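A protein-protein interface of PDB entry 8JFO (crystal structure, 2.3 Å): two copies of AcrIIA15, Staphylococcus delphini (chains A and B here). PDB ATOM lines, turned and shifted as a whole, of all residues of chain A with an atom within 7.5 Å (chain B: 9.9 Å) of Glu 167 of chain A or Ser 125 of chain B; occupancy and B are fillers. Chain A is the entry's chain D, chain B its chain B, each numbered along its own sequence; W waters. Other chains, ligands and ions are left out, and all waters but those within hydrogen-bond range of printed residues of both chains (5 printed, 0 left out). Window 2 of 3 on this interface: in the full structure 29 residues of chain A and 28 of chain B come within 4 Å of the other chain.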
ATOM      1  N   THR A  63       0.128  31.763  16.071  1.00  0.00           N
ATOM      2  CA  THR A  63      -0.165  31.525  17.473  1.00  0.00           C
ATOM      3  C   THR A  63      -1.660  31.688  17.701  1.00  0.00           C
ATOM      4  O   THR A  63      -2.235  32.704  17.301  1.00  0.00           O
ATOM      5  CB  THR A  63       0.607  32.480  18.384  1.00  0.00           C
ATOM      6  OG1 THR A  63       1.997  32.144  18.359  1.00  0.00           O
ATOM      7  CG2 THR A  63       0.101  32.377  19.803  1.00  0.00           C
ATOM      8  N   TRP A  64      -2.289  30.689  18.317  1.00  0.00           N
ATOM      9  CA  TRP A  64      -3.671  30.808  18.754  1.00  0.00           C
ATOM     10  C   TRP A  64      -3.704  30.346  20.203  1.00  0.00           C
ATOM     11  O   TRP A  64      -3.045  29.368  20.567  1.00  0.00           O
ATOM     12  CB  TRP A  64      -4.646  29.987  17.872  1.00  0.00           C
ATOM     13  CG  TRP A  64      -6.101  30.266  18.164  1.00  0.00           C
ATOM     14  CD1 TRP A  64      -6.971  29.464  18.850  1.00  0.00           C
ATOM     15  CD2 TRP A  64      -6.846  31.435  17.793  1.00  0.00           C
ATOM     16  NE1 TRP A  64      -8.206  30.057  18.920  1.00  0.00           N
ATOM     17  CE2 TRP A  64      -8.156  31.273  18.292  1.00  0.00           C
ATOM     18  CE3 TRP A  64      -6.530  32.607  17.094  1.00  0.00           C
ATOM     19  CZ2 TRP A  64      -9.161  32.232  18.101  1.00  0.00           C
ATOM     20  CZ3 TRP A  64      -7.525  33.565  16.911  1.00  0.00           C
ATOM     21  CH2 TRP A  64      -8.826  33.369  17.414  1.00  0.00           C
ATOM     22  N   ILE A  65      -4.470  31.056  21.023  1.00  0.00           N
ATOM     23  CA  ILE A  65      -4.534  30.866  22.462  1.00  0.00           C
ATOM     24  C   ILE A  65      -5.978  30.594  22.849  1.00  0.00           C
ATOM     25  O   ILE A  65      -6.886  31.337  22.446  1.00  0.00           O
ATOM     26  CB  ILE A  65      -4.031  32.110  23.209  1.00  0.00           C
ATOM     27  CG1 ILE A  65      -2.708  32.588  22.619  1.00  0.00           C
ATOM     28  CG2 ILE A  65      -3.971  31.842  24.736  1.00  0.00           C
ATOM     29  CD1 ILE A  65      -2.285  33.946  23.135  1.00  0.00           C
ATOM     30  N   VAL A  66      -6.179  29.538  23.629  1.00  0.00           N
ATOM     31  CA  VAL A  66      -7.460  29.222  24.240  1.00  0.00           C
ATOM     32  C   VAL A  66      -7.276  29.278  25.752  1.00  0.00           C
ATOM     33  O   VAL A  66      -6.477  28.523  26.313  1.00  0.00           O
ATOM     34  CB  VAL A  66      -7.975  27.841  23.802  1.00  0.00           C
ATOM     35  CG1 VAL A  66      -9.242  27.485  24.560  1.00  0.00           C
ATOM     36  CG2 VAL A  66      -8.223  27.809  22.280  1.00  0.00           C
ATOM     37  N   TYR A  67      -8.039  30.139  26.413  1.00  0.00           N
ATOM     38  CA  TYR A  67      -8.036  30.251  27.861  1.00  0.00           C
ATOM     39  C   TYR A  67      -9.242  29.518  28.429  1.00  0.00           C
ATOM     40  O   TYR A  67     -10.365  29.679  27.926  1.00  0.00           O
ATOM     41  CB  TYR A  67      -8.089  31.710  28.298  1.00  0.00           C
ATOM     42  CG  TYR A  67      -8.492  31.875  29.741  1.00  0.00           C
ATOM     43  CD1 TYR A  67      -7.564  31.693  30.763  1.00  0.00           C
ATOM     44  CD2 TYR A  67      -9.802  32.209  30.090  1.00  0.00           C
ATOM     45  CE1 TYR A  67      -7.928  31.850  32.090  1.00  0.00           C
ATOM     46  CE2 TYR A  67     -10.176  32.370  31.405  1.00  0.00           C
ATOM     47  CZ  TYR A  67      -9.240  32.188  32.405  1.00  0.00           C
ATOM     48  OH  TYR A  67      -9.613  32.345  33.722  1.00  0.00           O
ATOM     49  N   ARG A  68      -9.007  28.731  29.478  1.00  0.00           N
ATOM     50  CA  ARG A  68     -10.056  28.050  30.232  1.00  0.00           C
ATOM     51  C   ARG A  68      -9.924  28.432  31.697  1.00  0.00           C
ATOM     52  O   ARG A  68      -8.856  28.243  32.300  1.00  0.00           O
ATOM     53  CB  ARG A  68      -9.982  26.528  30.070  1.00  0.00           C
ATOM     54  CG  ARG A  68     -10.475  26.053  28.716  1.00  0.00           C
ATOM     55  CD  ARG A  68     -10.382  24.549  28.534  1.00  0.00           C
ATOM     56  NE  ARG A  68     -10.765  24.186  27.175  1.00  0.00           N
ATOM     57  CZ  ARG A  68      -9.908  23.976  26.184  1.00  0.00           C
ATOM     58  NH1 ARG A  68      -8.601  24.130  26.352  1.00  0.00           N
ATOM     59  NH2 ARG A  68     -10.376  23.665  24.980  1.00  0.00           N
ATOM     60  N   ALA A  80     -12.187  31.595  26.680  1.00  0.00           N
ATOM     61  CA  ALA A  80     -11.930  32.776  25.831  1.00  0.00           C
ATOM     62  C   ALA A  80     -10.838  32.420  24.825  1.00  0.00           C
ATOM     63  O   ALA A  80      -9.975  31.606  25.158  1.00  0.00           O
ATOM     64  CB  ALA A  80     -11.599  33.989  26.666  1.00  0.00           C
ATOM     65  N   GLY A  82      -8.236  33.768  21.247  1.00  0.00           N
ATOM     66  CA  GLY A  82      -7.595  34.911  20.589  1.00  0.00           C
ATOM     67  C   GLY A  82      -6.185  34.597  20.139  1.00  0.00           C
ATOM     68  O   GLY A  82      -5.632  33.592  20.593  1.00  0.00           O
ATOM     69  N   TYR A  85      -2.792  37.723  23.982  1.00  0.00           N
ATOM     70  CA  TYR A  85      -3.417  37.771  25.294  1.00  0.00           C
ATOM     71  C   TYR A  85      -4.400  38.928  25.410  1.00  0.00           C
ATOM     72  O   TYR A  85      -5.404  38.809  26.125  1.00  0.00           O
ATOM     73  CB  TYR A  85      -2.352  37.818  26.389  1.00  0.00           C
ATOM     74  CG  TYR A  85      -1.643  36.486  26.532  1.00  0.00           C
ATOM     75  CD1 TYR A  85      -2.329  35.351  26.959  1.00  0.00           C
ATOM     76  CD2 TYR A  85      -0.298  36.355  26.213  1.00  0.00           C
ATOM     77  CE1 TYR A  85      -1.684  34.121  27.079  1.00  0.00           C
ATOM     78  CE2 TYR A  85       0.352  35.140  26.322  1.00  0.00           C
ATOM     79  CZ  TYR A  85      -0.341  34.026  26.758  1.00  0.00           C
ATOM     80  OH  TYR A  85       0.322  32.825  26.870  1.00  0.00           O
ATOM     81  N   ARG A 151      -2.256  38.290  30.132  1.00  0.00           N
ATOM     82  CA  ARG A 151      -2.239  36.961  30.725  1.00  0.00           C
ATOM     83  C   ARG A 151      -2.175  37.052  32.243  1.00  0.00           C
ATOM     84  O   ARG A 151      -2.875  36.318  32.963  1.00  0.00           O
ATOM     85  CB  ARG A 151      -1.056  36.152  30.182  1.00  0.00           C
ATOM     86  CG  ARG A 151      -0.775  34.907  31.016  1.00  0.00           C
ATOM     87  CD  ARG A 151      -0.060  33.839  30.233  1.00  0.00           C
ATOM     88  NE  ARG A 151       0.178  32.661  31.054  1.00  0.00           N
ATOM     89  CZ  ARG A 151       0.703  31.531  30.604  1.00  0.00           C
ATOM     90  NH1 ARG A 151       1.077  31.398  29.343  1.00  0.00           N
ATOM     91  NH2 ARG A 151       0.870  30.514  31.446  1.00  0.00           N
ATOM     92  N   GLU A 165      -6.026  28.191  32.837  1.00  0.00           N
ATOM     93  CA  GLU A 165      -5.254  27.344  31.896  1.00  0.00           C
ATOM     94  C   GLU A 165      -5.149  28.031  30.532  1.00  0.00           C
ATOM     95  O   GLU A 165      -6.181  28.463  30.005  1.00  0.00           O
ATOM     96  CB  GLU A 165      -5.870  25.950  31.810  1.00  0.00           C
ATOM     97  N   PHE A 166      -3.936  28.110  29.993  1.00  0.00           N
ATOM     98  CA  PHE A 166      -3.720  28.716  28.660  1.00  0.00           C
ATOM     99  C   PHE A 166      -3.172  27.643  27.720  1.00  0.00           C
ATOM    100  O   PHE A 166      -2.048  27.172  27.934  1.00  0.00           O
ATOM    101  CB  PHE A 166      -2.826  29.955  28.751  1.00  0.00           C
ATOM    102  CG  PHE A 166      -3.431  31.166  29.412  1.00  0.00           C
ATOM    103  CD1 PHE A 166      -4.204  32.057  28.686  1.00  0.00           C
ATOM    104  CD2 PHE A 166      -3.205  31.431  30.752  1.00  0.00           C
ATOM    105  CE1 PHE A 166      -4.744  33.181  29.288  1.00  0.00           C
ATOM    106  CE2 PHE A 166      -3.752  32.552  31.354  1.00  0.00           C
ATOM    107  CZ  PHE A 166      -4.518  33.426  30.621  1.00  0.00           C
ATOM    108  N   GLU A 167      -3.962  27.263  26.725  1.00  0.00           N
ATOM    109  CA  GLU A 167      -3.550  26.268  25.755  1.00  0.00           C
ATOM    110  C   GLU A 167      -3.141  26.981  24.470  1.00  0.00           C
ATOM    111  O   GLU A 167      -3.946  27.703  23.871  1.00  0.00           O
ATOM    112  CB  GLU A 167      -4.697  25.295  25.522  1.00  0.00           C
ATOM    113  CG  GLU A 167      -4.468  24.265  24.487  1.00  0.00           C
ATOM    114  CD  GLU A 167      -5.795  23.732  23.966  1.00  0.00           C
ATOM    115  OE1 GLU A 167      -6.514  23.108  24.774  1.00  0.00           O
ATOM    116  OE2 GLU A 167      -6.115  23.934  22.769  1.00  0.00           O
ATOM    117  N   ILE A 168      -1.896  26.777  24.048  1.00  0.00           N
ATOM    118  CA  ILE A 168      -1.328  27.470  22.900  1.00  0.00           C
ATOM    119  C   ILE A 168      -1.144  26.472  21.769  1.00  0.00           C
ATOM    120  O   ILE A 168      -0.642  25.364  21.988  1.00  0.00           O
ATOM    121  CB  ILE A 168       0.017  28.139  23.244  1.00  0.00           C
ATOM    122  CG1 ILE A 168      -0.216  29.395  24.081  1.00  0.00           C
ATOM    123  CG2 ILE A 168       0.700  28.580  21.957  1.00  0.00           C
ATOM    124  CD1 ILE A 168      -0.375  29.173  25.505  1.00  0.00           C
ATOM    125  N   THR A 169      -1.580  26.866  20.569  1.00  0.00           N
ATOM    126  CA  THR A 169      -1.353  26.041  19.354  1.00  0.00           C
ATOM    127  C   THR A 169      -0.656  26.888  18.280  1.00  0.00           C
ATOM    128  O   THR A 169      -0.901  28.100  18.223  1.00  0.00           O
ATOM    129  CB  THR A 169      -2.619  25.356  18.820  1.00  0.00           C
ATOM    130  OG1 THR A 169      -2.199  24.499  17.760  1.00  0.00           O
ATOM    131  CG2 THR A 169      -3.662  26.329  18.318  1.00  0.00           C
ATOM    132  N   HIS A 170       0.215  26.262  17.495  1.00  0.00           N
ATOM    133  CA  HIS A 170       0.948  26.950  16.407  1.00  0.00           C
ATOM    134  C   HIS A 170       0.548  26.342  15.062  1.00  0.00           C
ATOM    135  O   HIS A 170       1.313  26.498  14.110  1.00  0.00           O
ATOM    136  CB  HIS A 170       2.450  26.879  16.677  1.00  0.00           C
ATOM    137  CG  HIS A 170       2.871  27.569  17.923  1.00  0.00           C
ATOM    138  ND1 HIS A 170       2.655  28.910  18.126  1.00  0.00           N
ATOM    139  CD2 HIS A 170       3.505  27.114  19.020  1.00  0.00           C
ATOM    140  CE1 HIS A 170       3.129  29.254  19.297  1.00  0.00           C
ATOM    141  NE2 HIS A 170       3.660  28.175  19.858  1.00  0.00           N
ATOM    142  N   GLU A 171      -0.595  25.660  15.007  1.00  0.00           N
ATOM    143  CA  GLU A 171      -1.084  25.022  13.753  1.00  0.00           C
ATOM    144  C   GLU A 171      -1.467  26.079  12.707  1.00  0.00           C
ATOM    145  O   GLU A 171      -1.527  27.268  13.063  1.00  0.00           O
ATOM    146  CB  GLU A 171      -2.261  24.092  14.054  1.00  0.00           C
ATOM    147  CG  GLU A 171      -3.502  24.803  14.559  1.00  0.00           C
ATOM    148  CD  GLU A 171      -4.542  23.878  15.166  1.00  0.00           C
ATOM    149  OE1 GLU A 171      -4.300  23.361  16.269  1.00  0.00           O
ATOM    150  OE2 GLU A 171      -5.592  23.673  14.531  1.00  0.00           O
ATOM    151  N   LEU B 101      10.296  25.383  26.146  1.00  0.00           N
ATOM    152  CA  LEU B 101       9.690  26.123  25.046  1.00  0.00           C
ATOM    153  C   LEU B 101       8.475  25.359  24.508  1.00  0.00           C
ATOM    154  O   LEU B 101       8.240  24.197  24.849  1.00  0.00           O
ATOM    155  CB  LEU B 101      10.720  26.379  23.939  1.00  0.00           C
ATOM    156  CG  LEU B 101      11.962  27.228  24.314  1.00  0.00           C
ATOM    157  CD1 LEU B 101      12.908  27.357  23.140  1.00  0.00           C
ATOM    158  CD2 LEU B 101      11.645  28.593  24.871  1.00  0.00           C
ATOM    159  N   ASP B 102       7.665  26.040  23.700  1.00  0.00           N
ATOM    160  CA  ASP B 102       6.424  25.448  23.202  1.00  0.00           C
ATOM    161  C   ASP B 102       6.700  24.132  22.478  1.00  0.00           C
ATOM    162  O   ASP B 102       7.748  23.957  21.852  1.00  0.00           O
ATOM    163  CB  ASP B 102       5.697  26.436  22.283  1.00  0.00           C
ATOM    164  CG  ASP B 102       5.033  27.561  23.063  1.00  0.00           C
ATOM    165  OD1 ASP B 102       5.327  27.654  24.281  1.00  0.00           O
ATOM    166  OD2 ASP B 102       4.238  28.343  22.467  1.00  0.00           O
ATOM    167  N   GLU B 103       5.752  23.194  22.582  1.00  0.00           N
ATOM    168  CA  GLU B 103       5.942  21.853  22.038  1.00  0.00           C
ATOM    169  C   GLU B 103       6.322  21.896  20.567  1.00  0.00           C
ATOM    170  O   GLU B 103       5.611  22.489  19.742  1.00  0.00           O
ATOM    171  CB  GLU B 103       4.659  21.034  22.204  1.00  0.00           C
ATOM    172  CG  GLU B 103       4.143  20.940  23.619  1.00  0.00           C
ATOM    173  CD  GLU B 103       5.090  20.186  24.535  1.00  0.00           C
ATOM    174  OE1 GLU B 103       5.610  19.115  24.126  1.00  0.00           O
ATOM    175  OE2 GLU B 103       5.312  20.669  25.665  1.00  0.00           O
ATOM    176  N   ASP B 104       7.452  21.252  20.252  1.00  0.00           N
ATOM    177  CA  ASP B 104       7.933  21.063  18.880  1.00  0.00           C
ATOM    178  C   ASP B 104       8.154  22.381  18.143  1.00  0.00           C
ATOM    179  O   ASP B 104       8.111  22.420  16.907  1.00  0.00           O
ATOM    180  CB  ASP B 104       6.984  20.159  18.085  1.00  0.00           C
ATOM    181  CG  ASP B 104       6.881  18.765  18.691  1.00  0.00           C
ATOM    182  OD1 ASP B 104       7.903  18.292  19.212  1.00  0.00           O
ATOM    183  OD2 ASP B 104       5.790  18.159  18.704  1.00  0.00           O
ATOM    184  N   ILE B 105       8.419  23.466  18.876  1.00  0.00           N
ATOM    185  CA  ILE B 105       8.525  24.773  18.224  1.00  0.00           C
ATOM    186  C   ILE B 105       9.642  24.779  17.182  1.00  0.00           C
ATOM    187  O   ILE B 105       9.482  25.348  16.099  1.00  0.00           O
ATOM    188  CB  ILE B 105       8.687  25.901  19.261  1.00  0.00           C
ATOM    189  CG1 ILE B 105       8.513  27.262  18.582  1.00  0.00           C
ATOM    190  CG2 ILE B 105      10.018  25.824  20.000  1.00  0.00           C
ATOM    191  CD1 ILE B 105       7.153  27.439  17.956  1.00  0.00           C
ATOM    192  N   ILE B 108       8.331  22.895  14.061  1.00  0.00           N
ATOM    193  CA  ILE B 108       7.257  23.651  13.422  1.00  0.00           C
ATOM    194  C   ILE B 108       7.826  24.845  12.672  1.00  0.00           C
ATOM    195  O   ILE B 108       7.436  25.129  11.533  1.00  0.00           O
ATOM    196  CB  ILE B 108       6.221  24.077  14.483  1.00  0.00           C
ATOM    197  CG1 ILE B 108       5.391  22.875  14.943  1.00  0.00           C
ATOM    198  CG2 ILE B 108       5.345  25.221  14.003  1.00  0.00           C
ATOM    199  CD1 ILE B 108       4.666  23.125  16.250  1.00  0.00           C
ATOM    200  N   TYR B 121       0.907  17.512   9.085  1.00  0.00           N
ATOM    201  CA  TYR B 121       1.659  17.042  10.232  1.00  0.00           C
ATOM    202  C   TYR B 121       0.812  16.936  11.493  1.00  0.00           C
ATOM    203  O   TYR B 121       1.350  16.619  12.559  1.00  0.00           O
ATOM    204  CB  TYR B 121       2.863  17.950  10.447  1.00  0.00           C
ATOM    205  CG  TYR B 121       3.831  17.865   9.296  1.00  0.00           C
ATOM    206  CD1 TYR B 121       3.645  18.625   8.139  1.00  0.00           C
ATOM    207  CD2 TYR B 121       4.922  17.002   9.348  1.00  0.00           C
ATOM    208  CE1 TYR B 121       4.526  18.538   7.073  1.00  0.00           C
ATOM    209  CE2 TYR B 121       5.817  16.912   8.287  1.00  0.00           C
ATOM    210  CZ  TYR B 121       5.612  17.679   7.157  1.00  0.00           C
ATOM    211  OH  TYR B 121       6.502  17.586   6.117  1.00  0.00           O
ATOM    212  N   ASP B 122      -0.500  17.161  11.387  1.00  0.00           N
ATOM    213  CA  ASP B 122      -1.423  17.025  12.514  1.00  0.00           C
ATOM    214  C   ASP B 122      -0.956  17.847  13.720  1.00  0.00           C
ATOM    215  O   ASP B 122      -0.805  17.340  14.834  1.00  0.00           O
ATOM    216  CB  ASP B 122      -1.601  15.552  12.895  1.00  0.00           C
ATOM    217  CG  ASP B 122      -2.178  14.717  11.762  1.00  0.00           C
ATOM    218  OD1 ASP B 122      -2.837  15.299  10.865  1.00  0.00           O
ATOM    219  OD2 ASP B 122      -1.956  13.477  11.762  1.00  0.00           O
ATOM    220  N   VAL B 123      -0.667  19.119  13.479  1.00  0.00           N
ATOM    221  CA  VAL B 123      -0.208  19.996  14.547  1.00  0.00           C
ATOM    222  C   VAL B 123      -1.381  20.422  15.422  1.00  0.00           C
ATOM    223  O   VAL B 123      -2.457  20.764  14.924  1.00  0.00           O
ATOM    224  CB  VAL B 123       0.527  21.212  13.964  1.00  0.00           C
ATOM    225  CG1 VAL B 123       0.898  22.180  15.074  1.00  0.00           C
ATOM    226  CG2 VAL B 123       1.773  20.763  13.199  1.00  0.00           C
ATOM    227  N   ASP B 124      -1.185  20.376  16.737  1.00  0.00           N
ATOM    228  CA  ASP B 124      -2.147  20.907  17.698  1.00  0.00           C
ATOM    229  C   ASP B 124      -1.354  21.411  18.910  1.00  0.00           C
ATOM    230  O   ASP B 124      -0.134  21.582  18.842  1.00  0.00           O
ATOM    231  CB  ASP B 124      -3.269  19.892  17.987  1.00  0.00           C
ATOM    232  CG  ASP B 124      -2.785  18.618  18.649  1.00  0.00           C
ATOM    233  OD1 ASP B 124      -1.647  18.568  19.174  1.00  0.00           O
ATOM    234  OD2 ASP B 124      -3.574  17.647  18.644  1.00  0.00           O
ATOM    235  N   SER B 125      -2.054  21.725  20.003  1.00  0.00           N
ATOM    236  CA  SER B 125      -1.373  22.208  21.202  1.00  0.00           C
ATOM    237  C   SER B 125      -0.311  21.227  21.701  1.00  0.00           C
ATOM    238  O   SER B 125       0.661  21.645  22.343  1.00  0.00           O
ATOM    239  CB  SER B 125      -2.380  22.521  22.309  1.00  0.00           C
ATOM    240  OG  SER B 125      -3.297  21.462  22.495  1.00  0.00           O
ATOM    241  N   ASP B 126      -0.488  19.924  21.456  1.00  0.00           N
ATOM    242  CA  ASP B 126       0.518  18.939  21.853  1.00  0.00           C
ATOM    243  C   ASP B 126       1.746  18.938  20.956  1.00  0.00           C
ATOM    244  O   ASP B 126       2.701  18.216  21.257  1.00  0.00           O
ATOM    245  CB  ASP B 126      -0.054  17.513  21.879  1.00  0.00           C
ATOM    246  CG  ASP B 126      -1.236  17.380  22.811  1.00  0.00           C
ATOM    247  OD1 ASP B 126      -1.176  17.939  23.934  1.00  0.00           O
ATOM    248  OD2 ASP B 126      -2.214  16.698  22.436  1.00  0.00           O
ATOM    249  N   GLY B 127       1.713  19.639  19.830  1.00  0.00           N
ATOM    250  CA  GLY B 127       2.870  19.685  18.957  1.00  0.00           C
ATOM    251  C   GLY B 127       2.556  18.992  17.652  1.00  0.00           C
ATOM    252  O   GLY B 127       1.400  18.954  17.217  1.00  0.00           O
ATOM    253  N   ILE B 128       3.585  18.454  17.011  1.00  0.00           N
ATOM    254  CA  ILE B 128       3.412  17.631  15.820  1.00  0.00           C
ATOM    255  C   ILE B 128       2.971  16.235  16.246  1.00  0.00           C
ATOM    256  O   ILE B 128       3.523  15.664  17.195  1.00  0.00           O
ATOM    257  CB  ILE B 128       4.706  17.578  15.001  1.00  0.00           C
ATOM    258  CG1 ILE B 128       5.076  18.986  14.538  1.00  0.00           C
ATOM    259  CG2 ILE B 128       4.533  16.625  13.816  1.00  0.00           C
ATOM    260  CD1 ILE B 128       6.482  19.132  14.039  1.00  0.00           C
ATOM    261  N   ASN B 129       1.896  15.736  15.635  1.00  0.00           N
ATOM    262  CA  ASN B 129       1.412  14.394  15.945  1.00  0.00           C
ATOM    263  C   ASN B 129       1.719  13.355  14.875  1.00  0.00           C
ATOM    264  O   ASN B 129       1.800  12.165  15.195  1.00  0.00           O
ATOM    265  CB  ASN B 129      -0.087  14.436  16.230  1.00  0.00           C
ATOM    266  CG  ASN B 129      -0.391  15.208  17.489  1.00  0.00           C
ATOM    267  OD1 ASN B 129      -0.226  14.702  18.598  1.00  0.00           O
ATOM    268  ND2 ASN B 129      -0.799  16.451  17.329  1.00  0.00           N
ATOM    269  N   TYR B 131       4.253  11.773  13.229  1.00  0.00           N
ATOM    270  CA  TYR B 131       5.700  11.588  13.273  1.00  0.00           C
ATOM    271  C   TYR B 131       6.243  10.986  11.984  1.00  0.00           C
ATOM    272  O   TYR B 131       7.409  11.224  11.642  1.00  0.00           O
ATOM    273  CB  TYR B 131       6.079  10.741  14.481  1.00  0.00           C
ATOM    274  CG  TYR B 131       5.671  11.405  15.768  1.00  0.00           C
ATOM    275  CD1 TYR B 131       6.340  12.537  16.212  1.00  0.00           C
ATOM    276  CD2 TYR B 131       4.605  10.924  16.528  1.00  0.00           C
ATOM    277  CE1 TYR B 131       5.978  13.172  17.387  1.00  0.00           C
ATOM    278  CE2 TYR B 131       4.234  11.557  17.713  1.00  0.00           C
ATOM    279  CZ  TYR B 131       4.935  12.683  18.133  1.00  0.00           C
ATOM    280  OH  TYR B 131       4.609  13.340  19.299  1.00  0.00           O
ATOM    281  N   SER B 158       4.705  30.741  23.961  1.00  0.00           N
ATOM    282  CA  SER B 158       3.812  31.392  24.902  1.00  0.00           C
ATOM    283  C   SER B 158       3.285  30.478  25.984  1.00  0.00           C
ATOM    284  O   SER B 158       2.570  30.962  26.862  1.00  0.00           O
ATOM    285  CB  SER B 158       2.617  32.017  24.169  1.00  0.00           C
ATOM    286  OG  SER B 158       2.293  33.252  24.767  1.00  0.00           O
ATOM    287  N   SER B 159       3.566  29.178  25.937  1.00  0.00           N
ATOM    288  CA  SER B 159       2.950  28.247  26.923  1.00  0.00           C
ATOM    289  C   SER B 159       3.507  28.447  28.338  1.00  0.00           C
ATOM    290  O   SER B 159       2.722  28.786  29.228  1.00  0.00           O
ATOM    291  CB  SER B 159       3.026  26.817  26.476  1.00  0.00           C
ATOM    292  OG  SER B 159       2.209  25.993  27.288  1.00  0.00           O
ATOM    293  N   GLN B 160       4.806  28.233  28.532  1.00  0.00           N
ATOM    294  CA  GLN B 160       5.436  28.368  29.874  1.00  0.00           C
ATOM    295  C   GLN B 160       6.157  29.711  29.953  1.00  0.00           C
ATOM    296  O   GLN B 160       5.975  30.411  30.950  1.00  0.00           O
ATOM    297  CB  GLN B 160       6.372  27.186  30.112  1.00  0.00           C
ATOM    298  CG  GLN B 160       5.724  25.843  29.811  1.00  0.00           C
ATOM    299  CD  GLN B 160       6.682  24.688  29.962  1.00  0.00           C
ATOM    300  OE1 GLN B 160       7.563  24.694  30.816  1.00  0.00           O
ATOM    301  NE2 GLN B 160       6.509  23.679  29.125  1.00  0.00           N
HETATM  302  O   HOH W   1       1.797  24.165  22.210  1.00  0.00           O
HETATM  303  O   HOH W   2       0.408  27.512  29.616  1.00  0.00           O
HETATM  304  O   HOH W   3       0.089  25.055  25.621  1.00  0.00           O
HETATM  305  O   HOH W   4      -5.556  20.441  15.139  1.00  0.00           O
HETATM  306  O   HOH W   5       1.115  23.899  17.997  1.00  0.00           O
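The side-chain carboxylate (OD2) of Asp 102 of chain B sits at hydrogen-bond distance from the backbone NH (N) of Ser 158 of chain B, 2.9 Å away. NH1 of Arg 68 of chain A is in salt-bridge range of OE1 of Glu 167 of chain A, 2.8 Å away. OH of Tyr 85 of chain A sits at hydrogen-bond distance from NH1 of Arg 151 of chain A (3.0 Å).
Water W2 lies within hydrogen-bond range of the backbone carbonyl oxygen (O) of Ser 159 of chain B (2.7 Å) and the backbone carbonyl oxygen (O) of Phe 166 of chain A (3.0 Å). Water W1 lies within hydrogen-bond range of O of Ile 168 of chain A (2.7 Å) and O of Ser 125 of chain B (2.8 Å). Water W4 bridges O of Val 123 of chain B and OE2 of Glu 171 of chain A.
No residue of chain B comes within 4 Å of Val 66 of chain A. Of chain B, only Ser 125 comes within 4 Å of Glu 167 of chain A. Of chain B, only Asp 102 (3.6 Å), Ser 125 (3.3 Å), Ser 158 (3.7 Å) and Ser 159 (3.7 Å) come within 4 Å of Ile 168 of chain A. Of the printed residues of chain B, His 170 of chain A touches Asp 102 (2.7 Å) and Ile 105 (3.8 Å). Asn 129 of chain B touches none of the printed residues of chain A. Of the printed residues of chain A, Ser 158 of chain B touches Tyr 85 (2.9 Å), Arg 151 (2.9 Å) and Ile 168 (3.7 Å). The nearest residue of chain B that does not touch Glu 167 of chain A is Ser 159 of chain B (6.0 Å). The nearest residue of chain A that does not touch Ser 125 of chain B is Glu 171 of chain A (4.7 Å).
No position is printed for both chains.
Among the printed residues, merely in contact across the chains: Ile 168 of chain A with Ser 125 of chain B (3.3 Å), Thr 169 of chain A with Asp 124 of chain B (3.4 Å), Glu 167 of chain A with Ser 125 of chain B (3.5 Å), Glu 171 of chain A with Asp 124 of chain B (3.6 Å), Thr 169 of chain A with Ser 125 of chain B (3.6 Å), Ile 168 of chain A with Asp 102 of chain B (3.6 Å), Ile 168 of chain A with Ser 158 of chain B (3.7 Å), Ile 168 of chain A with Ser 159 of chain B (3.7 Å) and His 170 of chain A with Ile 105 of chain B (3.8 Å).
OD2 of Asp 102 of chain B is in hydrogen-bond range of NE2 of His 170 of chain A, at 2.7 Å. The side-chain hydroxyl (OG) of Ser 158 of chain B sits at hydrogen-bond distance from the side-chain hydroxyl (OH) of Tyr 85 of chain A (2.9 Å). The backbone carbonyl oxygen (O) of Ser 158 of chain B sits at hydrogen-bond distance from the guanidinium group (NH1) of Arg 151 of chain A, at 2.9 Å. NH1 of Arg 151 of chain A sits at hydrogen-bond distance from O of Ser 159 of chain B, 3.1 Å away. OE1 of Glu 171 of chain A sits close to O of Val 123 of chain B, 3.5 Å away.
Hydrophobic or aromatic side chains of chain A that line the printed part of chain B: Tyr 85, Ile 168 and His 170. Of the 19 printed residues of chain B, 7 touch a printed residue of chain A. Printed residues of chain B that touch a printed residue of chain A: Asp 102, Ile 105, Val 123, Asp 124, Ser 125, Ser 158 and Ser 159. Hydrophobic or aromatic side chains of chain B within 4 Å of the printed part of chain A: Ile 105 and Val 123. Among the printed residues, 14 pairs touch across the chains. Among the printed residues, no Asp or Glu carboxylate lies within 4 Å of a Lys or Arg side-chain nitrogen of the other chain.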
